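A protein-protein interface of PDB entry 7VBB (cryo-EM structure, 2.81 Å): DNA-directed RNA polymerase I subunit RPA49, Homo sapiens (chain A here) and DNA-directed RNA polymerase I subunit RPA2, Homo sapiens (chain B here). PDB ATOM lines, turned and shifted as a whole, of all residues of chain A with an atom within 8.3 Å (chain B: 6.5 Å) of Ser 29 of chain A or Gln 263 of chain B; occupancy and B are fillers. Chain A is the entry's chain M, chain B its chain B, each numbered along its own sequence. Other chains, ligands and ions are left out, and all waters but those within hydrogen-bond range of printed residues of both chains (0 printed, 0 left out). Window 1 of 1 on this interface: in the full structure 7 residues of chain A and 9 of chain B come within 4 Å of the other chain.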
ATOM      1  N   VAL A  26     -24.514   3.614  15.318  1.00  0.00           N
ATOM      2  CA  VAL A  26     -25.081   4.819  14.721  1.00  0.00           C
ATOM      3  C   VAL A  26     -26.113   5.429  15.668  1.00  0.00           C
ATOM      4  O   VAL A  26     -26.793   4.709  16.404  1.00  0.00           O
ATOM      5  CB  VAL A  26     -25.728   4.524  13.348  1.00  0.00           C
ATOM      6  CG1 VAL A  26     -24.681   4.022  12.356  1.00  0.00           C
ATOM      7  CG2 VAL A  26     -26.857   3.506  13.499  1.00  0.00           C
ATOM      8  N   GLN A  27     -26.076   6.720  15.703  1.00  0.00           N
ATOM      9  CA  GLN A  27     -27.054   7.526  16.423  1.00  0.00           C
ATOM     10  C   GLN A  27     -27.619   8.630  15.535  1.00  0.00           C
ATOM     11  O   GLN A  27     -26.866   9.383  14.917  1.00  0.00           O
ATOM     12  CB  GLN A  27     -26.426   8.135  17.680  1.00  0.00           C
ATOM     13  CG  GLN A  27     -27.414   8.894  18.555  1.00  0.00           C
ATOM     14  CD  GLN A  27     -26.773   9.465  19.806  1.00  0.00           C
ATOM     15  OE1 GLN A  27     -25.610   9.878  19.790  1.00  0.00           O
ATOM     16  NE2 GLN A  27     -27.526   9.491  20.900  1.00  0.00           N
ATOM     17  N   PHE A  28     -28.925   8.756  15.481  1.00  0.00           N
ATOM     18  CA  PHE A  28     -29.586   9.742  14.635  1.00  0.00           C
ATOM     19  C   PHE A  28     -29.897  11.010  15.421  1.00  0.00           C
ATOM     20  O   PHE A  28     -30.446  10.944  16.523  1.00  0.00           O
ATOM     21  CB  PHE A  28     -30.873   9.163  14.038  1.00  0.00           C
ATOM     22  CG  PHE A  28     -30.637   8.075  13.028  1.00  0.00           C
ATOM     23  CD1 PHE A  28     -30.475   6.756  13.438  1.00  0.00           C
ATOM     24  CD2 PHE A  28     -30.581   8.365  11.671  1.00  0.00           C
ATOM     25  CE1 PHE A  28     -30.260   5.744  12.507  1.00  0.00           C
ATOM     26  CE2 PHE A  28     -30.365   7.356  10.733  1.00  0.00           C
ATOM     27  CZ  PHE A  28     -30.205   6.046  11.158  1.00  0.00           C
ATOM     28  N   SER A  29     -29.541  12.149  14.966  1.00  0.00           N
ATOM     29  CA  SER A  29     -29.704  13.426  15.652  1.00  0.00           C
ATOM     30  C   SER A  29     -31.177  13.779  15.824  1.00  0.00           C
ATOM     31  O   SER A  29     -31.539  14.523  16.737  1.00  0.00           O
ATOM     32  CB  SER A  29     -28.990  14.541  14.884  1.00  0.00           C
ATOM     33  OG  SER A  29     -29.476  14.627  13.556  1.00  0.00           O
ATOM     34  N   ASN A  30     -32.079  13.259  14.976  1.00  0.00           N
ATOM     35  CA  ASN A  30     -33.483  13.653  15.013  1.00  0.00           C
ATOM     36  C   ASN A  30     -34.357  12.562  15.626  1.00  0.00           C
ATOM     37  O   ASN A  30     -35.554  12.487  15.344  1.00  0.00           O
ATOM     38  CB  ASN A  30     -33.981  14.006  13.609  1.00  0.00           C
ATOM     39  CG  ASN A  30     -33.281  15.217  13.029  1.00  0.00           C
ATOM     40  OD1 ASN A  30     -32.885  16.130  13.759  1.00  0.00           O
ATOM     41  ND2 ASN A  30     -33.124  15.239  11.711  1.00  0.00           N
ATOM     42  N   GLY A  31     -33.733  11.695  16.376  1.00  0.00           N
ATOM     43  CA  GLY A  31     -34.537  10.670  17.021  1.00  0.00           C
ATOM     44  C   GLY A  31     -34.260   9.276  16.492  1.00  0.00           C
ATOM     45  O   GLY A  31     -33.120   8.948  16.158  1.00  0.00           O
ATOM     46  N   LYS A  32     -35.309   8.372  16.654  1.00  0.00           N
ATOM     47  CA  LYS A  32     -35.211   6.961  16.290  1.00  0.00           C
ATOM     48  C   LYS A  32     -35.859   6.698  14.933  1.00  0.00           C
ATOM     49  O   LYS A  32     -36.818   7.376  14.555  1.00  0.00           O
ATOM     50  CB  LYS A  32     -35.862   6.085  17.361  1.00  0.00           C
ATOM     51  CG  LYS A  32     -35.665   4.591  17.141  1.00  0.00           C
ATOM     52  CD  LYS A  32     -36.294   3.774  18.261  1.00  0.00           C
ATOM     53  CE  LYS A  32     -36.152   2.278  18.012  1.00  0.00           C
ATOM     54  NZ  LYS A  32     -36.795   1.473  19.094  1.00  0.00           N
ATOM     55  N   TYR A  69     -28.813  10.253   5.223  1.00  0.00           N
ATOM     56  CA  TYR A  69     -28.112  10.615   6.451  1.00  0.00           C
ATOM     57  C   TYR A  69     -26.612  10.380   6.311  1.00  0.00           C
ATOM     58  O   TYR A  69     -26.186   9.428   5.654  1.00  0.00           O
ATOM     59  CB  TYR A  69     -28.657   9.816   7.638  1.00  0.00           C
ATOM     60  CG  TYR A  69     -30.110  10.092   7.938  1.00  0.00           C
ATOM     61  CD1 TYR A  69     -31.118   9.459   7.221  1.00  0.00           C
ATOM     62  CD2 TYR A  69     -30.477  10.984   8.943  1.00  0.00           C
ATOM     63  CE1 TYR A  69     -32.461   9.708   7.494  1.00  0.00           C
ATOM     64  CE2 TYR A  69     -31.814  11.240   9.226  1.00  0.00           C
ATOM     65  CZ  TYR A  69     -32.798  10.598   8.496  1.00  0.00           C
ATOM     66  OH  TYR A  69     -34.123  10.848   8.772  1.00  0.00           O
ATOM     67  N   VAL A  70     -25.891  11.340   6.926  1.00  0.00           N
ATOM     68  CA  VAL A  70     -24.444  11.180   6.850  1.00  0.00           C
ATOM     69  C   VAL A  70     -23.823  11.426   8.223  1.00  0.00           C
ATOM     70  O   VAL A  70     -24.271  12.301   8.966  1.00  0.00           O
ATOM     71  CB  VAL A  70     -23.820  12.135   5.805  1.00  0.00           C
ATOM     72  CG1 VAL A  70     -22.296  12.033   5.820  1.00  0.00           C
ATOM     73  CG2 VAL A  70     -24.365  11.831   4.412  1.00  0.00           C
ATOM     74  N   LEU A  79     -17.985  14.339  16.918  1.00  0.00           N
ATOM     75  CA  LEU A  79     -18.332  14.973  18.196  1.00  0.00           C
ATOM     76  C   LEU A  79     -17.320  14.560  19.270  1.00  0.00           C
ATOM     77  O   LEU A  79     -16.467  13.713  18.970  1.00  0.00           O
ATOM     78  CB  LEU A  79     -19.793  14.631  18.473  1.00  0.00           C
ATOM     79  CG  LEU A  79     -20.793  15.499  17.709  1.00  0.00           C
ATOM     80  CD1 LEU A  79     -22.178  15.438  18.337  1.00  0.00           C
ATOM     81  CD2 LEU A  79     -20.314  16.942  17.651  1.00  0.00           C
ATOM     82  N   PHE A 107     -21.142   6.759  15.109  1.00  0.00           N
ATOM     83  CA  PHE A 107     -21.432   7.764  14.093  1.00  0.00           C
ATOM     84  C   PHE A 107     -22.732   8.493  14.407  1.00  0.00           C
ATOM     85  O   PHE A 107     -23.777   7.863  14.587  1.00  0.00           O
ATOM     86  CB  PHE A 107     -21.516   7.121  12.705  1.00  0.00           C
ATOM     87  CG  PHE A 107     -20.190   6.634  12.181  1.00  0.00           C
ATOM     88  CD1 PHE A 107     -19.703   5.386  12.543  1.00  0.00           C
ATOM     89  CD2 PHE A 107     -19.433   7.425  11.328  1.00  0.00           C
ATOM     90  CE1 PHE A 107     -18.479   4.932  12.062  1.00  0.00           C
ATOM     91  CE2 PHE A 107     -18.207   6.978  10.840  1.00  0.00           C
ATOM     92  CZ  PHE A 107     -17.732   5.729  11.211  1.00  0.00           C
ATOM     93  N   ASN A 108     -22.670   9.786  14.507  1.00  0.00           N
ATOM     94  CA  ASN A 108     -23.876  10.601  14.624  1.00  0.00           C
ATOM     95  C   ASN A 108     -24.435  10.972  13.253  1.00  0.00           C
ATOM     96  O   ASN A 108     -23.806  11.720  12.503  1.00  0.00           O
ATOM     97  CB  ASN A 108     -23.593  11.863  15.442  1.00  0.00           C
ATOM     98  CG  ASN A 108     -23.282  11.559  16.895  1.00  0.00           C
ATOM     99  OD1 ASN A 108     -23.898  10.683  17.505  1.00  0.00           O
ATOM    100  ND2 ASN A 108     -22.321  12.282  17.458  1.00  0.00           N
ATOM    101  N   MET A 109     -25.592  10.429  13.003  1.00  0.00           N
ATOM    102  CA  MET A 109     -26.170  10.568  11.669  1.00  0.00           C
ATOM    103  C   MET A 109     -26.978  11.857  11.555  1.00  0.00           C
ATOM    104  O   MET A 109     -27.855  12.119  12.384  1.00  0.00           O
ATOM    105  CB  MET A 109     -27.055   9.365  11.338  1.00  0.00           C
ATOM    106  CG  MET A 109     -26.337   8.028  11.444  1.00  0.00           C
ATOM    107  SD  MET A 109     -24.925   7.896  10.280  1.00  0.00           S
ATOM    108  CE  MET A 109     -25.816   7.781   8.705  1.00  0.00           C
ATOM    109  N   GLN A 110     -26.912  12.392  10.291  1.00  0.00           N
ATOM    110  CA  GLN A 110     -27.578  13.683   9.916  1.00  0.00           C
ATOM    111  C   GLN A 110     -28.093  13.738   8.452  1.00  0.00           C
ATOM    112  O   GLN A 110     -27.371  13.286   7.588  1.00  0.00           O
ATOM    113  CB  GLN A 110     -26.496  14.758   9.866  1.00  0.00           C
ATOM    114  CG  GLN A 110     -26.342  15.550  11.150  1.00  0.00           C
ATOM    115  CD  GLN A 110     -26.898  16.940  10.975  1.00  0.00           C
ATOM    116  OE1 GLN A 110     -26.797  17.533   9.904  1.00  0.00           O
ATOM    117  NE2 GLN A 110     -27.491  17.466  12.034  1.00  0.00           N
ATOM    118  N   PRO A 111     -29.213  14.432   8.101  1.00  0.00           N
ATOM    119  CA  PRO A 111     -29.807  14.546   6.710  1.00  0.00           C
ATOM    120  C   PRO A 111     -29.062  15.193   5.523  1.00  0.00           C
ATOM    121  O   PRO A 111     -28.404  16.188   5.759  1.00  0.00           O
ATOM    122  CB  PRO A 111     -31.044  15.424   6.904  1.00  0.00           C
ATOM    123  CG  PRO A 111     -31.412  15.195   8.341  1.00  0.00           C
ATOM    124  CD  PRO A 111     -30.077  15.141   9.051  1.00  0.00           C
ATOM    125  N   SER B 258     -24.714  23.416  12.357  1.00  0.00           N
ATOM    126  CA  SER B 258     -25.405  22.832  11.183  1.00  0.00           C
ATOM    127  C   SER B 258     -26.156  21.588  11.638  1.00  0.00           C
ATOM    128  O   SER B 258     -25.768  20.489  11.239  1.00  0.00           O
ATOM    129  CB  SER B 258     -24.435  22.480  10.117  1.00  0.00           C
ATOM    130  OG  SER B 258     -23.407  21.656  10.639  1.00  0.00           O
ATOM    131  N   PHE B 259     -27.194  21.779  12.442  1.00  0.00           N
ATOM    132  CA  PHE B 259     -27.969  20.651  13.001  1.00  0.00           C
ATOM    133  C   PHE B 259     -29.414  20.889  12.599  1.00  0.00           C
ATOM    134  O   PHE B 259     -29.772  22.038  12.312  1.00  0.00           O
ATOM    135  CB  PHE B 259     -28.049  20.713  14.524  1.00  0.00           C
ATOM    136  CG  PHE B 259     -26.917  20.183  15.362  1.00  0.00           C
ATOM    137  CD1 PHE B 259     -25.824  19.554  14.801  1.00  0.00           C
ATOM    138  CD2 PHE B 259     -26.976  20.302  16.742  1.00  0.00           C
ATOM    139  CE1 PHE B 259     -24.806  19.068  15.606  1.00  0.00           C
ATOM    140  CE2 PHE B 259     -25.961  19.814  17.545  1.00  0.00           C
ATOM    141  CZ  PHE B 259     -24.875  19.196  16.974  1.00  0.00           C
ATOM    142  N   SER B 260     -30.223  19.847  12.646  1.00  0.00           N
ATOM    143  CA  SER B 260     -31.631  19.915  12.236  1.00  0.00           C
ATOM    144  C   SER B 260     -32.366  20.757  13.255  1.00  0.00           C
ATOM    145  O   SER B 260     -31.834  20.918  14.345  1.00  0.00           O
ATOM    146  CB  SER B 260     -32.111  18.549  12.318  1.00  0.00           C
ATOM    147  OG  SER B 260     -31.129  17.734  12.929  1.00  0.00           O
ATOM    148  N   ASP B 261     -33.543  21.277  12.932  1.00  0.00           N
ATOM    149  CA  ASP B 261     -34.324  22.001  13.957  1.00  0.00           C
ATOM    150  C   ASP B 261     -34.693  21.052  15.095  1.00  0.00           C
ATOM    151  O   ASP B 261     -34.786  21.540  16.197  1.00  0.00           O
ATOM    152  CB  ASP B 261     -35.486  22.757  13.346  1.00  0.00           C
ATOM    153  CG  ASP B 261     -35.100  24.161  12.925  1.00  0.00           C
ATOM    154  OD1 ASP B 261     -34.107  24.666  13.468  1.00  0.00           O
ATOM    155  OD2 ASP B 261     -35.792  24.736  12.061  1.00  0.00           O
ATOM    156  N   TYR B 262     -34.981  19.785  14.834  1.00  0.00           N
ATOM    157  CA  TYR B 262     -35.389  18.881  15.924  1.00  0.00           C
ATOM    158  C   TYR B 262     -34.242  18.665  16.874  1.00  0.00           C
ATOM    159  O   TYR B 262     -34.496  18.659  18.056  1.00  0.00           O
ATOM    160  CB  TYR B 262     -35.670  17.469  15.455  1.00  0.00           C
ATOM    161  CG  TYR B 262     -36.283  16.572  16.498  1.00  0.00           C
ATOM    162  CD1 TYR B 262     -37.343  16.986  17.277  1.00  0.00           C
ATOM    163  CD2 TYR B 262     -35.801  15.297  16.700  1.00  0.00           C
ATOM    164  CE1 TYR B 262     -37.910  16.153  18.227  1.00  0.00           C
ATOM    165  CE2 TYR B 262     -36.352  14.448  17.640  1.00  0.00           C
ATOM    166  CZ  TYR B 262     -37.411  14.878  18.408  1.00  0.00           C
ATOM    167  OH  TYR B 262     -37.942  14.029  19.334  1.00  0.00           O
ATOM    168  N   GLN B 263     -33.029  18.479  16.387  1.00  0.00           N
ATOM    169  CA  GLN B 263     -31.861  18.342  17.298  1.00  0.00           C
ATOM    170  C   GLN B 263     -31.608  19.623  18.099  1.00  0.00           C
ATOM    171  O   GLN B 263     -31.358  19.503  19.285  1.00  0.00           O
ATOM    172  CB  GLN B 263     -30.644  17.809  16.564  1.00  0.00           C
ATOM    173  CG  GLN B 263     -29.592  17.225  17.483  1.00  0.00           C
ATOM    174  CD  GLN B 263     -28.305  17.067  16.719  1.00  0.00           C
ATOM    175  OE1 GLN B 263     -28.224  17.413  15.546  1.00  0.00           O
ATOM    176  NE2 GLN B 263     -27.296  16.523  17.374  1.00  0.00           N
ATOM    177  N   ILE B 264     -31.702  20.803  17.508  1.00  0.00           N
ATOM    178  CA  ILE B 264     -31.600  22.043  18.324  1.00  0.00           C
ATOM    179  C   ILE B 264     -32.676  21.988  19.413  1.00  0.00           C
ATOM    180  O   ILE B 264     -32.359  22.296  20.545  1.00  0.00           O
ATOM    181  CB  ILE B 264     -31.739  23.282  17.431  1.00  0.00           C
ATOM    182  CG1 ILE B 264     -30.532  23.449  16.513  1.00  0.00           C
ATOM    183  CG2 ILE B 264     -31.984  24.527  18.261  1.00  0.00           C
ATOM    184  CD1 ILE B 264     -30.688  24.565  15.519  1.00  0.00           C
ATOM    185  N   PHE B 265     -33.896  21.561  19.105  1.00  0.00           N
ATOM    186  CA  PHE B 265     -35.045  21.507  20.045  1.00  0.00           C
ATOM    187  C   PHE B 265     -34.812  20.466  21.113  1.00  0.00           C
ATOM    188  O   PHE B 265     -35.008  20.752  22.264  1.00  0.00           O
ATOM    189  CB  PHE B 265     -36.274  21.076  19.252  1.00  0.00           C
ATOM    190  CG  PHE B 265     -37.493  20.566  19.975  1.00  0.00           C
ATOM    191  CD1 PHE B 265     -38.532  21.419  20.290  1.00  0.00           C
ATOM    192  CD2 PHE B 265     -37.650  19.219  20.239  1.00  0.00           C
ATOM    193  CE1 PHE B 265     -39.667  20.949  20.923  1.00  0.00           C
ATOM    194  CE2 PHE B 265     -38.786  18.748  20.873  1.00  0.00           C
ATOM    195  CZ  PHE B 265     -39.792  19.615  21.209  1.00  0.00           C
ATOM    196  N   GLN B 266     -34.347  19.302  20.729  1.00  0.00           N
ATOM    197  CA  GLN B 266     -34.178  18.213  21.699  1.00  0.00           C
ATOM    198  C   GLN B 266     -33.193  18.719  22.756  1.00  0.00           C
ATOM    199  O   GLN B 266     -33.285  18.218  23.873  1.00  0.00           O
ATOM    200  CB  GLN B 266     -33.913  16.926  20.925  1.00  0.00           C
ATOM    201  CG  GLN B 266     -33.003  15.935  21.621  1.00  0.00           C
ATOM    202  CD  GLN B 266     -32.775  14.772  20.692  1.00  0.00           C
ATOM    203  OE1 GLN B 266     -33.625  14.449  19.868  1.00  0.00           O
ATOM    204  NE2 GLN B 266     -31.618  14.141  20.811  1.00  0.00           N
ATOM    205  N   GLU B 267     -32.244  19.601  22.414  1.00  0.00           N
ATOM    206  CA  GLU B 267     -31.293  20.243  23.371  1.00  0.00           C
ATOM    207  C   GLU B 267     -31.928  21.283  24.304  1.00  0.00           C
ATOM    208  O   GLU B 267     -31.529  21.317  25.458  1.00  0.00           O
ATOM    209  CB  GLU B 267     -30.067  20.820  22.668  1.00  0.00           C
ATOM    210  CG  GLU B 267     -28.947  19.817  22.462  1.00  0.00           C
ATOM    211  CD  GLU B 267     -29.014  18.967  21.202  1.00  0.00           C
ATOM    212  OE1 GLU B 267     -29.720  17.940  21.213  1.00  0.00           O
ATOM    213  OE2 GLU B 267     -28.352  19.329  20.212  1.00  0.00           O
ATOM    214  N   LEU B 268     -32.836  22.139  23.855  1.00  0.00           N
ATOM    215  CA  LEU B 268     -33.360  23.203  24.752  1.00  0.00           C
ATOM    216  C   LEU B 268     -34.466  22.657  25.659  1.00  0.00           C
ATOM    217  O   LEU B 268     -34.982  23.437  26.447  1.00  0.00           O
ATOM    218  CB  LEU B 268     -33.877  24.390  23.943  1.00  0.00           C
ATOM    219  CG  LEU B 268     -32.919  25.077  22.984  1.00  0.00           C
ATOM    220  CD1 LEU B 268     -33.643  25.419  21.695  1.00  0.00           C
ATOM    221  CD2 LEU B 268     -32.406  26.349  23.610  1.00  0.00           C
ATOM    222  N   LYS B 270     -34.031  19.671  27.350  1.00  0.00           N
ATOM    223  CA  LYS B 270     -33.348  18.468  27.878  1.00  0.00           C
ATOM    224  C   LYS B 270     -33.941  18.042  29.214  1.00  0.00           C
ATOM    225  O   LYS B 270     -34.331  16.884  29.317  1.00  0.00           O
ATOM    226  CB  LYS B 270     -31.834  18.678  27.915  1.00  0.00           C
ATOM    227  CG  LYS B 270     -30.973  17.540  27.402  1.00  0.00           C
ATOM    228  CD  LYS B 270     -30.701  17.599  25.924  1.00  0.00           C
ATOM    229  CE  LYS B 270     -29.476  16.807  25.524  1.00  0.00           C
ATOM    230  NZ  LYS B 270     -29.395  16.612  24.058  1.00  0.00           N
ATOM    231  N   PHE B 343     -22.788  26.974  20.986  1.00  0.00           N
ATOM    232  CA  PHE B 343     -24.204  26.545  20.934  1.00  0.00           C
ATOM    233  C   PHE B 343     -24.622  25.920  22.257  1.00  0.00           C
ATOM    234  O   PHE B 343     -25.606  26.367  22.807  1.00  0.00           O
ATOM    235  CB  PHE B 343     -24.403  25.497  19.842  1.00  0.00           C
ATOM    236  CG  PHE B 343     -25.729  24.786  19.821  1.00  0.00           C
ATOM    237  CD1 PHE B 343     -26.870  25.425  19.379  1.00  0.00           C
ATOM    238  CD2 PHE B 343     -25.825  23.460  20.196  1.00  0.00           C
ATOM    239  CE1 PHE B 343     -28.083  24.762  19.348  1.00  0.00           C
ATOM    240  CE2 PHE B 343     -27.037  22.797  20.164  1.00  0.00           C
ATOM    241  CZ  PHE B 343     -28.164  23.450  19.738  1.00  0.00           C
ATOM    242  N   TYR B 344     -23.856  24.991  22.796  1.00  0.00           N
ATOM    243  CA  TYR B 344     -24.263  24.301  24.028  1.00  0.00           C
ATOM    244  C   TYR B 344     -24.327  25.302  25.185  1.00  0.00           C
ATOM    245  O   TYR B 344     -25.118  25.083  26.090  1.00  0.00           O
ATOM    246  CB  TYR B 344     -23.387  23.079  24.233  1.00  0.00           C
ATOM    247  CG  TYR B 344     -23.680  21.894  23.352  1.00  0.00           C
ATOM    248  CD1 TYR B 344     -24.839  21.158  23.506  1.00  0.00           C
ATOM    249  CD2 TYR B 344     -22.772  21.476  22.402  1.00  0.00           C
ATOM    250  CE1 TYR B 344     -25.101  20.052  22.718  1.00  0.00           C
ATOM    251  CE2 TYR B 344     -23.015  20.372  21.606  1.00  0.00           C
ATOM    252  CZ  TYR B 344     -24.184  19.656  21.765  1.00  0.00           C
ATOM    253  OH  TYR B 344     -24.428  18.563  20.987  1.00  0.00           O
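Ser 29 of chain A touches three residues of chain B. Gln 263 of chain B touches three residues of chain A. Printed residues of chain A within 4 Å of Gln 266 of chain B: Ser 29. Of the printed residues of chain A, Ser 258 of chain B touches Gln 110 (3.4 Å). Printed residues of chain A within 4 Å of Ser 260 of chain B: Ser 29 (3.6 Å), Asn 30 (2.5 Å) and Gln 110 (3.7 Å). The nearest residue of chain B that does not touch Ser 29 of chain A is Tyr 262 of chain B (4.3 Å).
The backbone NH (N) of Ser 29 of chain A lies within hydrogen-bond range of the backbone carbonyl oxygen (O) of Met 109 of chain A, 3.1 Å away. The backbone NH (N) of Val 70 of chain A sits at hydrogen-bond distance from the backbone carbonyl oxygen (O) of Gln 110 of chain A (2.5 Å).
Of the 15 printed residues of chain A, 3 touch a printed residue of chain B. Printed residues of chain A that touch a printed residue of chain B: Ser 29, Asn 30 and Gln 110. Hydrophobic or aromatic side chains of chain B that line the printed part of chain A: Phe 259 and Tyr 262.
OE1 of Gln 110 of chain A lies close to O of Ser 258 of chain B. OG of Ser 260 of chain B sits at hydrogen-bond distance from OD1 of Asn 30 of chain A, 2.5 Å away.
Among the printed residues, pairs that only touch across the chains: Ser 29 of chain A with Ser 260 of chain B, Ser 29 of chain A with Gln 263 of chain B, Ser 29 of chain A with Gln 266 of chain B, Asn 30 of chain A with Tyr 262 of chain B, Asn 30 of chain A with Gln 263 of chain B, Gln 110 of chain A with Phe 259 of chain B, Gln 110 of chain A with Ser 260 of chain B and Gln 110 of chain A with Gln 263 of chain B.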
